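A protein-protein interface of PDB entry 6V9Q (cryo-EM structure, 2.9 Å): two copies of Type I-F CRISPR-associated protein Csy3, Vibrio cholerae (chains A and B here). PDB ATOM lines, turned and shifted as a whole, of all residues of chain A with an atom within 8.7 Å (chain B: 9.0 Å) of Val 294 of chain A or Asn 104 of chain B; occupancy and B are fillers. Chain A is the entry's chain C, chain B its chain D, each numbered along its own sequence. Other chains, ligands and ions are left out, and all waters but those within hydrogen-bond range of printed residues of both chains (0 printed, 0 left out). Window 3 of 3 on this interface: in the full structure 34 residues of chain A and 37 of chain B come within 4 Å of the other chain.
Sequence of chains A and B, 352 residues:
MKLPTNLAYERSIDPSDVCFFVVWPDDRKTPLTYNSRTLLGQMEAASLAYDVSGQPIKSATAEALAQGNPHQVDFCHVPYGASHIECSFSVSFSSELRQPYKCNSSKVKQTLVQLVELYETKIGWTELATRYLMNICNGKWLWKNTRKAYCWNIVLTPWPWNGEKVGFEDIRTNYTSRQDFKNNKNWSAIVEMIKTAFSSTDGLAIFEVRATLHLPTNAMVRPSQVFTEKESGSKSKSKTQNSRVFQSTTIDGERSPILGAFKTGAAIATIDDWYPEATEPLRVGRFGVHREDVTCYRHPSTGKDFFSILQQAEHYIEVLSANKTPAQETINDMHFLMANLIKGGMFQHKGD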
ATOM      1  N   VAL A 289      21.528 -17.304 -15.978  1.00  0.00           N
ATOM      2  CA  VAL A 289      20.114 -17.016 -15.876  1.00  0.00           C
ATOM      3  C   VAL A 289      19.497 -17.905 -14.809  1.00  0.00           C
ATOM      4  O   VAL A 289      20.039 -18.942 -14.422  1.00  0.00           O
ATOM      5  CB  VAL A 289      19.398 -17.195 -17.228  1.00  0.00           C
ATOM      6  CG1 VAL A 289      20.193 -16.560 -18.328  1.00  0.00           C
ATOM      7  CG2 VAL A 289      19.131 -18.632 -17.527  1.00  0.00           C
ATOM      8  N   HIS A 290      18.340 -17.478 -14.325  1.00  0.00           N
ATOM      9  CA  HIS A 290      17.595 -18.174 -13.284  1.00  0.00           C
ATOM     10  C   HIS A 290      16.152 -18.136 -13.752  1.00  0.00           C
ATOM     11  O   HIS A 290      15.484 -17.118 -13.599  1.00  0.00           O
ATOM     12  CB  HIS A 290      17.766 -17.488 -11.940  1.00  0.00           C
ATOM     13  CG  HIS A 290      17.110 -18.198 -10.802  1.00  0.00           C
ATOM     14  ND1 HIS A 290      16.945 -17.611  -9.568  1.00  0.00           N
ATOM     15  CD2 HIS A 290      16.586 -19.440 -10.700  1.00  0.00           C
ATOM     16  CE1 HIS A 290      16.348 -18.461  -8.755  1.00  0.00           C
ATOM     17  NE2 HIS A 290      16.116 -19.577  -9.419  1.00  0.00           N
ATOM     18  N   ARG A 291      15.679 -19.219 -14.346  1.00  0.00           N
ATOM     19  CA  ARG A 291      14.419 -19.109 -15.054  1.00  0.00           C
ATOM     20  C   ARG A 291      13.209 -19.326 -14.150  1.00  0.00           C
ATOM     21  O   ARG A 291      12.074 -19.223 -14.625  1.00  0.00           O
ATOM     22  CB  ARG A 291      14.411 -20.052 -16.264  1.00  0.00           C
ATOM     23  CG  ARG A 291      13.888 -21.439 -16.067  1.00  0.00           C
ATOM     24  CD  ARG A 291      14.792 -22.354 -15.326  1.00  0.00           C
ATOM     25  NE  ARG A 291      14.094 -23.623 -15.191  1.00  0.00           N
ATOM     26  CZ  ARG A 291      13.276 -23.910 -14.184  1.00  0.00           C
ATOM     27  NH1 ARG A 291      12.650 -25.074 -14.126  1.00  0.00           N
ATOM     28  NH2 ARG A 291      13.106 -23.031 -13.210  1.00  0.00           N
ATOM     29  N   GLU A 292      13.426 -19.591 -12.857  1.00  0.00           N
ATOM     30  CA  GLU A 292      12.355 -19.490 -11.870  1.00  0.00           C
ATOM     31  C   GLU A 292      11.807 -18.073 -11.827  1.00  0.00           C
ATOM     32  O   GLU A 292      10.655 -17.824 -12.185  1.00  0.00           O
ATOM     33  CB  GLU A 292      12.875 -19.878 -10.487  1.00  0.00           C
ATOM     34  CG  GLU A 292      13.325 -21.312 -10.329  1.00  0.00           C
ATOM     35  CD  GLU A 292      12.178 -22.293 -10.259  1.00  0.00           C
ATOM     36  OE1 GLU A 292      11.135 -21.952  -9.665  1.00  0.00           O
ATOM     37  OE2 GLU A 292      12.319 -23.404 -10.812  1.00  0.00           O
ATOM     38  N   ASP A 293      12.633 -17.128 -11.415  1.00  0.00           N
ATOM     39  CA  ASP A 293      12.302 -15.712 -11.452  1.00  0.00           C
ATOM     40  C   ASP A 293      13.032 -15.086 -12.629  1.00  0.00           C
ATOM     41  O   ASP A 293      14.230 -14.815 -12.547  1.00  0.00           O
ATOM     42  CB  ASP A 293      12.651 -15.047 -10.123  1.00  0.00           C
ATOM     43  CG  ASP A 293      13.988 -15.486  -9.580  1.00  0.00           C
ATOM     44  OD1 ASP A 293      14.609 -16.368 -10.188  1.00  0.00           O
ATOM     45  OD2 ASP A 293      14.414 -14.961  -8.536  1.00  0.00           O
ATOM     46  N   VAL A 294      12.287 -14.772 -13.689  1.00  0.00           N
ATOM     47  CA  VAL A 294      12.838 -14.741 -15.038  1.00  0.00           C
ATOM     48  C   VAL A 294      13.706 -13.502 -15.193  1.00  0.00           C
ATOM     49  O   VAL A 294      13.246 -12.446 -15.637  1.00  0.00           O
ATOM     50  CB  VAL A 294      11.702 -14.752 -16.077  1.00  0.00           C
ATOM     51  CG1 VAL A 294      12.234 -14.906 -17.489  1.00  0.00           C
ATOM     52  CG2 VAL A 294      10.713 -15.826 -15.745  1.00  0.00           C
ATOM     53  N   THR A 295      14.975 -13.641 -14.812  1.00  0.00           N
ATOM     54  CA  THR A 295      15.967 -12.578 -14.859  1.00  0.00           C
ATOM     55  C   THR A 295      17.329 -13.192 -15.107  1.00  0.00           C
ATOM     56  O   THR A 295      17.514 -14.405 -15.025  1.00  0.00           O
ATOM     57  CB  THR A 295      16.072 -11.762 -13.559  1.00  0.00           C
ATOM     58  OG1 THR A 295      16.254 -12.641 -12.442  1.00  0.00           O
ATOM     59  CG2 THR A 295      14.900 -10.820 -13.342  1.00  0.00           C
ATOM     60  N   CYS A 296      18.289 -12.326 -15.382  1.00  0.00           N
ATOM     61  CA  CYS A 296      19.690 -12.699 -15.432  1.00  0.00           C
ATOM     62  C   CYS A 296      20.394 -12.107 -14.225  1.00  0.00           C
ATOM     63  O   CYS A 296      20.469 -10.884 -14.079  1.00  0.00           O
ATOM     64  CB  CYS A 296      20.361 -12.201 -16.711  1.00  0.00           C
ATOM     65  SG  CYS A 296      19.793 -12.932 -18.232  1.00  0.00           S
ATOM     66  N   TYR A 297      20.898 -12.969 -13.361  1.00  0.00           N
ATOM     67  CA  TYR A 297      22.064 -12.578 -12.601  1.00  0.00           C
ATOM     68  C   TYR A 297      23.257 -12.644 -13.543  1.00  0.00           C
ATOM     69  O   TYR A 297      23.179 -13.259 -14.611  1.00  0.00           O
ATOM     70  CB  TYR A 297      22.240 -13.488 -11.393  1.00  0.00           C
ATOM     71  CG  TYR A 297      21.052 -13.436 -10.468  1.00  0.00           C
ATOM     72  CD1 TYR A 297      20.901 -12.399  -9.564  1.00  0.00           C
ATOM     73  CD2 TYR A 297      20.065 -14.409 -10.521  1.00  0.00           C
ATOM     74  CE1 TYR A 297      19.808 -12.339  -8.729  1.00  0.00           C
ATOM     75  CE2 TYR A 297      18.967 -14.358  -9.693  1.00  0.00           C
ATOM     76  CZ  TYR A 297      18.844 -13.324  -8.800  1.00  0.00           C
ATOM     77  OH  TYR A 297      17.750 -13.275  -7.971  1.00  0.00           O
ATOM     78  N   LYS B   2      -1.004  -5.404 -10.022  1.00  0.00           N
ATOM     79  CA  LYS B   2      -1.236  -5.890 -11.372  1.00  0.00           C
ATOM     80  C   LYS B   2      -0.739  -7.324 -11.510  1.00  0.00           C
ATOM     81  O   LYS B   2       0.142  -7.776 -10.777  1.00  0.00           O
ATOM     82  CB  LYS B   2      -0.558  -4.968 -12.394  1.00  0.00           C
ATOM     83  CG  LYS B   2       0.971  -4.861 -12.292  1.00  0.00           C
ATOM     84  CD  LYS B   2       1.724  -5.726 -13.316  1.00  0.00           C
ATOM     85  CE  LYS B   2       3.234  -5.517 -13.237  1.00  0.00           C
ATOM     86  NZ  LYS B   2       3.992  -6.384 -14.185  1.00  0.00           N
ATOM     87  N   LEU B   3      -1.319  -8.038 -12.455  1.00  0.00           N
ATOM     88  CA  LEU B   3      -0.817  -9.380 -12.697  1.00  0.00           C
ATOM     89  C   LEU B   3       0.431  -9.312 -13.572  1.00  0.00           C
ATOM     90  O   LEU B   3       0.450  -8.576 -14.561  1.00  0.00           O
ATOM     91  CB  LEU B   3      -1.876 -10.253 -13.375  1.00  0.00           C
ATOM     92  CG  LEU B   3      -2.919 -11.008 -12.542  1.00  0.00           C
ATOM     93  CD1 LEU B   3      -2.232 -11.936 -11.578  1.00  0.00           C
ATOM     94  CD2 LEU B   3      -3.880 -10.098 -11.802  1.00  0.00           C
ATOM     95  N   PRO B   4       1.485 -10.049 -13.229  1.00  0.00           N
ATOM     96  CA  PRO B   4       2.691 -10.062 -14.061  1.00  0.00           C
ATOM     97  C   PRO B   4       2.460 -10.792 -15.373  1.00  0.00           C
ATOM     98  O   PRO B   4       1.426 -11.418 -15.607  1.00  0.00           O
ATOM     99  CB  PRO B   4       3.708 -10.805 -13.197  1.00  0.00           C
ATOM    100  CG  PRO B   4       3.210 -10.679 -11.833  1.00  0.00           C
ATOM    101  CD  PRO B   4       1.725 -10.686 -11.931  1.00  0.00           C
ATOM    102  N   THR B   5       3.456 -10.703 -16.247  1.00  0.00           N
ATOM    103  CA  THR B   5       3.375 -11.425 -17.507  1.00  0.00           C
ATOM    104  C   THR B   5       3.683 -12.905 -17.351  1.00  0.00           C
ATOM    105  O   THR B   5       3.392 -13.678 -18.266  1.00  0.00           O
ATOM    106  CB  THR B   5       4.322 -10.820 -18.544  1.00  0.00           C
ATOM    107  OG1 THR B   5       5.672 -10.968 -18.102  1.00  0.00           O
ATOM    108  CG2 THR B   5       4.028  -9.351 -18.738  1.00  0.00           C
ATOM    109  N   ASN B   6       4.260 -13.315 -16.226  1.00  0.00           N
ATOM    110  CA  ASN B   6       4.551 -14.716 -15.952  1.00  0.00           C
ATOM    111  C   ASN B   6       4.233 -14.966 -14.488  1.00  0.00           C
ATOM    112  O   ASN B   6       4.888 -14.399 -13.616  1.00  0.00           O
ATOM    113  CB  ASN B   6       6.011 -15.051 -16.248  1.00  0.00           C
ATOM    114  CG  ASN B   6       6.323 -15.065 -17.723  1.00  0.00           C
ATOM    115  OD1 ASN B   6       5.564 -15.602 -18.521  1.00  0.00           O
ATOM    116  ND2 ASN B   6       7.450 -14.479 -18.094  1.00  0.00           N
ATOM    117  N   LEU B   7       3.232 -15.795 -14.212  1.00  0.00           N
ATOM    118  CA  LEU B   7       2.980 -16.219 -12.841  1.00  0.00           C
ATOM    119  C   LEU B   7       2.306 -17.577 -12.910  1.00  0.00           C
ATOM    120  O   LEU B   7       1.275 -17.711 -13.569  1.00  0.00           O
ATOM    121  CB  LEU B   7       2.118 -15.206 -12.085  1.00  0.00           C
ATOM    122  CG  LEU B   7       2.240 -15.166 -10.559  1.00  0.00           C
ATOM    123  CD1 LEU B   7       1.856 -13.816 -10.082  1.00  0.00           C
ATOM    124  CD2 LEU B   7       1.374 -16.147  -9.875  1.00  0.00           C
ATOM    125  N   ALA B   8       2.881 -18.577 -12.245  1.00  0.00           N
ATOM    126  CA  ALA B   8       2.356 -19.933 -12.281  1.00  0.00           C
ATOM    127  C   ALA B   8       2.836 -20.679 -11.053  1.00  0.00           C
ATOM    128  O   ALA B   8       3.932 -20.424 -10.557  1.00  0.00           O
ATOM    129  CB  ALA B   8       2.797 -20.670 -13.545  1.00  0.00           C
ATOM    130  N   PRO B 100       6.312 -19.154  -5.723  1.00  0.00           N
ATOM    131  CA  PRO B 100       5.823 -19.356  -7.087  1.00  0.00           C
ATOM    132  C   PRO B 100       6.782 -20.193  -7.909  1.00  0.00           C
ATOM    133  O   PRO B 100       8.002 -20.116  -7.757  1.00  0.00           O
ATOM    134  CB  PRO B 100       5.718 -17.934  -7.643  1.00  0.00           C
ATOM    135  CG  PRO B 100       5.593 -17.083  -6.467  1.00  0.00           C
ATOM    136  CD  PRO B 100       6.451 -17.719  -5.426  1.00  0.00           C
ATOM    137  N   TYR B 101       6.207 -21.012  -8.789  1.00  0.00           N
ATOM    138  CA  TYR B 101       7.016 -21.799  -9.714  1.00  0.00           C
ATOM    139  C   TYR B 101       7.697 -20.919 -10.750  1.00  0.00           C
ATOM    140  O   TYR B 101       8.782 -21.255 -11.228  1.00  0.00           O
ATOM    141  CB  TYR B 101       6.145 -22.851 -10.397  1.00  0.00           C
ATOM    142  CG  TYR B 101       6.853 -23.691 -11.430  1.00  0.00           C
ATOM    143  CD1 TYR B 101       7.719 -24.704 -11.053  1.00  0.00           C
ATOM    144  CD2 TYR B 101       6.651 -23.474 -12.783  1.00  0.00           C
ATOM    145  CE1 TYR B 101       8.364 -25.469 -11.991  1.00  0.00           C
ATOM    146  CE2 TYR B 101       7.297 -24.230 -13.727  1.00  0.00           C
ATOM    147  CZ  TYR B 101       8.148 -25.228 -13.325  1.00  0.00           C
ATOM    148  OH  TYR B 101       8.793 -25.993 -14.262  1.00  0.00           O
ATOM    149  N   LYS B 102       7.088 -19.792 -11.098  1.00  0.00           N
ATOM    150  CA  LYS B 102       7.614 -18.930 -12.144  1.00  0.00           C
ATOM    151  C   LYS B 102       7.013 -17.555 -11.937  1.00  0.00           C
ATOM    152  O   LYS B 102       5.794 -17.435 -11.889  1.00  0.00           O
ATOM    153  CB  LYS B 102       7.257 -19.484 -13.521  1.00  0.00           C
ATOM    154  CG  LYS B 102       7.872 -18.783 -14.702  1.00  0.00           C
ATOM    155  CD  LYS B 102       7.494 -19.530 -15.964  1.00  0.00           C
ATOM    156  CE  LYS B 102       7.938 -18.822 -17.230  1.00  0.00           C
ATOM    157  NZ  LYS B 102       9.410 -18.840 -17.416  1.00  0.00           N
ATOM    158  N   CYS B 103       7.855 -16.531 -11.786  1.00  0.00           N
ATOM    159  CA  CYS B 103       7.352 -15.175 -11.562  1.00  0.00           C
ATOM    160  C   CYS B 103       8.434 -14.179 -11.944  1.00  0.00           C
ATOM    161  O   CYS B 103       9.450 -14.088 -11.252  1.00  0.00           O
ATOM    162  CB  CYS B 103       6.934 -14.987 -10.111  1.00  0.00           C
ATOM    163  SG  CYS B 103       6.142 -13.421  -9.765  1.00  0.00           S
ATOM    164  N   ASN B 104       8.204 -13.402 -13.002  1.00  0.00           N
ATOM    165  CA  ASN B 104       9.210 -12.452 -13.459  1.00  0.00           C
ATOM    166  C   ASN B 104       9.256 -11.165 -12.647  1.00  0.00           C
ATOM    167  O   ASN B 104      10.181 -10.371 -12.836  1.00  0.00           O
ATOM    168  CB  ASN B 104       9.005 -12.115 -14.937  1.00  0.00           C
ATOM    169  CG  ASN B 104       7.641 -11.551 -15.233  1.00  0.00           C
ATOM    170  OD1 ASN B 104       6.791 -11.437 -14.359  1.00  0.00           O
ATOM    171  ND2 ASN B 104       7.434 -11.160 -16.476  1.00  0.00           N
ATOM    172  N   SER B 105       8.298 -10.930 -11.763  1.00  0.00           N
ATOM    173  CA  SER B 105       8.260  -9.728 -10.942  1.00  0.00           C
ATOM    174  C   SER B 105       8.704 -10.088  -9.533  1.00  0.00           C
ATOM    175  O   SER B 105       8.138 -10.992  -8.916  1.00  0.00           O
ATOM    176  CB  SER B 105       6.861  -9.122 -10.932  1.00  0.00           C
ATOM    177  OG  SER B 105       6.810  -7.963 -10.123  1.00  0.00           O
ATOM    178  N   SER B 106       9.716  -9.385  -9.027  1.00  0.00           N
ATOM    179  CA  SER B 106      10.220  -9.674  -7.692  1.00  0.00           C
ATOM    180  C   SER B 106       9.362  -9.068  -6.594  1.00  0.00           C
ATOM    181  O   SER B 106       9.429  -9.530  -5.454  1.00  0.00           O
ATOM    182  CB  SER B 106      11.658  -9.182  -7.543  1.00  0.00           C
ATOM    183  OG  SER B 106      11.717  -7.772  -7.603  1.00  0.00           O
ATOM    184  N   LYS B 107       8.563  -8.046  -6.904  1.00  0.00           N
ATOM    185  CA  LYS B 107       7.652  -7.501  -5.903  1.00  0.00           C
ATOM    186  C   LYS B 107       6.473  -8.430  -5.673  1.00  0.00           C
ATOM    187  O   LYS B 107       5.985  -8.557  -4.545  1.00  0.00           O
ATOM    188  CB  LYS B 107       7.160  -6.121  -6.327  1.00  0.00           C
ATOM    189  CG  LYS B 107       8.255  -5.092  -6.449  1.00  0.00           C
ATOM    190  CD  LYS B 107       8.873  -4.788  -5.096  1.00  0.00           C
ATOM    191  CE  LYS B 107       9.923  -3.698  -5.205  1.00  0.00           C
ATOM    192  NZ  LYS B 107      10.568  -3.413  -3.896  1.00  0.00           N
ATOM    193  N   VAL B 108       5.999  -9.082  -6.729  1.00  0.00           N
ATOM    194  CA  VAL B 108       4.867  -9.985  -6.600  1.00  0.00           C
ATOM    195  C   VAL B 108       5.298 -11.292  -5.943  1.00  0.00           C
ATOM    196  O   VAL B 108       4.514 -11.919  -5.221  1.00  0.00           O
ATOM    197  CB  VAL B 108       4.244 -10.195  -7.988  1.00  0.00           C
ATOM    198  CG1 VAL B 108       3.017 -11.046  -7.919  1.00  0.00           C
ATOM    199  CG2 VAL B 108       3.909  -8.859  -8.605  1.00  0.00           C
ATOM    200  N   LYS B 109       6.528 -11.726  -6.223  1.00  0.00           N
ATOM    201  CA  LYS B 109       7.046 -12.965  -5.588  1.00  0.00           C
ATOM    202  C   LYS B 109       7.153 -12.735  -4.078  1.00  0.00           C
ATOM    203  O   LYS B 109       6.732 -13.621  -3.316  1.00  0.00           O
ATOM    204  CB  LYS B 109       8.419 -13.326  -6.161  1.00  0.00           C
ATOM    205  CG  LYS B 109       9.179 -14.385  -5.375  1.00  0.00           C
ATOM    206  CD  LYS B 109      10.494 -14.773  -6.006  1.00  0.00           C
ATOM    207  CE  LYS B 109      11.332 -15.664  -5.116  1.00  0.00           C
ATOM    208  NZ  LYS B 109      10.574 -16.855  -4.667  1.00  0.00           N
ATOM    209  N   GLN B 348      -1.501 -15.849 -15.396  1.00  0.00           N
ATOM    210  CA  GLN B 348      -1.110 -14.745 -16.263  1.00  0.00           C
ATOM    211  C   GLN B 348      -2.329 -14.001 -16.792  1.00  0.00           C
ATOM    212  O   GLN B 348      -3.448 -14.129 -16.292  1.00  0.00           O
ATOM    213  CB  GLN B 348      -0.265 -15.212 -17.442  1.00  0.00           C
ATOM    214  CG  GLN B 348       1.095 -15.728 -17.109  1.00  0.00           C
ATOM    215  CD  GLN B 348       1.148 -17.218 -17.081  1.00  0.00           C
ATOM    216  OE1 GLN B 348       0.289 -17.882 -17.651  1.00  0.00           O
ATOM    217  NE2 GLN B 348       2.170 -17.762 -16.439  1.00  0.00           N
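Val 294 of chain A touches just these residues of chain B: Lys 102 (3.7 Å), Cys 103 (3.8 Å) and Asn 104 (3.9 Å).
Thr 295 of chain A touches none of the printed residues of chain B.
Printed residues of chain B within 4 Å of Arg 291 of chain A: Tyr 101 and Lys 102.
Printed residues of chain B within 4 Å of Asp 293 of chain A: Cys 103 (3.3 Å).
Lys 109 of chain B touches none of the printed residues of chain A.
Cys 296 of chain A touches none of the printed residues of chain B.
The nearest residue of chain B that does not touch Val 294 of chain A is Asn 6 of chain B (4.2 Å).
Arg 291 of chain A touches Tyr 101 of chain B.
Arg 291 of chain A touches Lys 102 of chain B (O to NZ, 3.9 Å).
O of Glu 292 of chain A touches CA of Lys 102 of chain B (3.2 Å).
Asp 293 of chain A touches Cys 103 of chain B.
Val 294 of chain A touches Lys 102 of chain B.
Val 294 of chain A touches Cys 103 of chain B (N to O, 3.8 Å).
CA of Asn 104 of chain B touches N of Val 294 of chain A, at 3.9 Å.
The side-chain hydroxyl (OG1) of Thr 5 of chain B is in hydrogen-bond range of the side-chain amide nitrogen (ND2) of Asn 104 of chain B.
The side-chain sulfur of Cys 103 of chain B sits at hydrogen-bond distance from the backbone carbonyl oxygen of Ser 105 of chain B (3.3 Å).
The backbone carbonyl oxygen (O) of Ala 8 of chain B lies within hydrogen-bond range of the backbone NH (N) of Tyr 101 of chain B, at 2.9 Å.
ND1 of His 290 of chain A sits at hydrogen-bond distance from OD1 of Asp 293 of chain A (2.7 Å).
The guanidinium group (NH2) of Arg 291 of chain A is in salt-bridge range of the side-chain carboxylate (OE2) of Glu 292 of chain A (2.6 Å).
The backbone carbonyl oxygen (O) of Lys 102 of chain B sits at hydrogen-bond distance from the backbone NH (N) of Ala 8 of chain B (3.1 Å).
No position is printed for both chains.
Of the 9 pairs that touch across the chains among the printed residues, none has its exchanged pair printed and touching as well.
O of Glu 292 of chain A sits at hydrogen-bond distance from N of Cys 103 of chain B (3.1 Å).
The backbone carbonyl oxygen of Tyr 101 of chain B sits close to the side-chain carboxylate of Glu 292 of chain A, at 2.9 Å.
Of the 9 printed residues of chain A, 4 touch a printed residue of chain B.
Printed residues of chain A that touch a printed residue of chain B: Arg 291, Glu 292, Asp 293 and Val 294.
Among the printed residues, no Asp or Glu carboxylate lies within 4 Å of a Lys or Arg side-chain nitrogen of the other chain.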
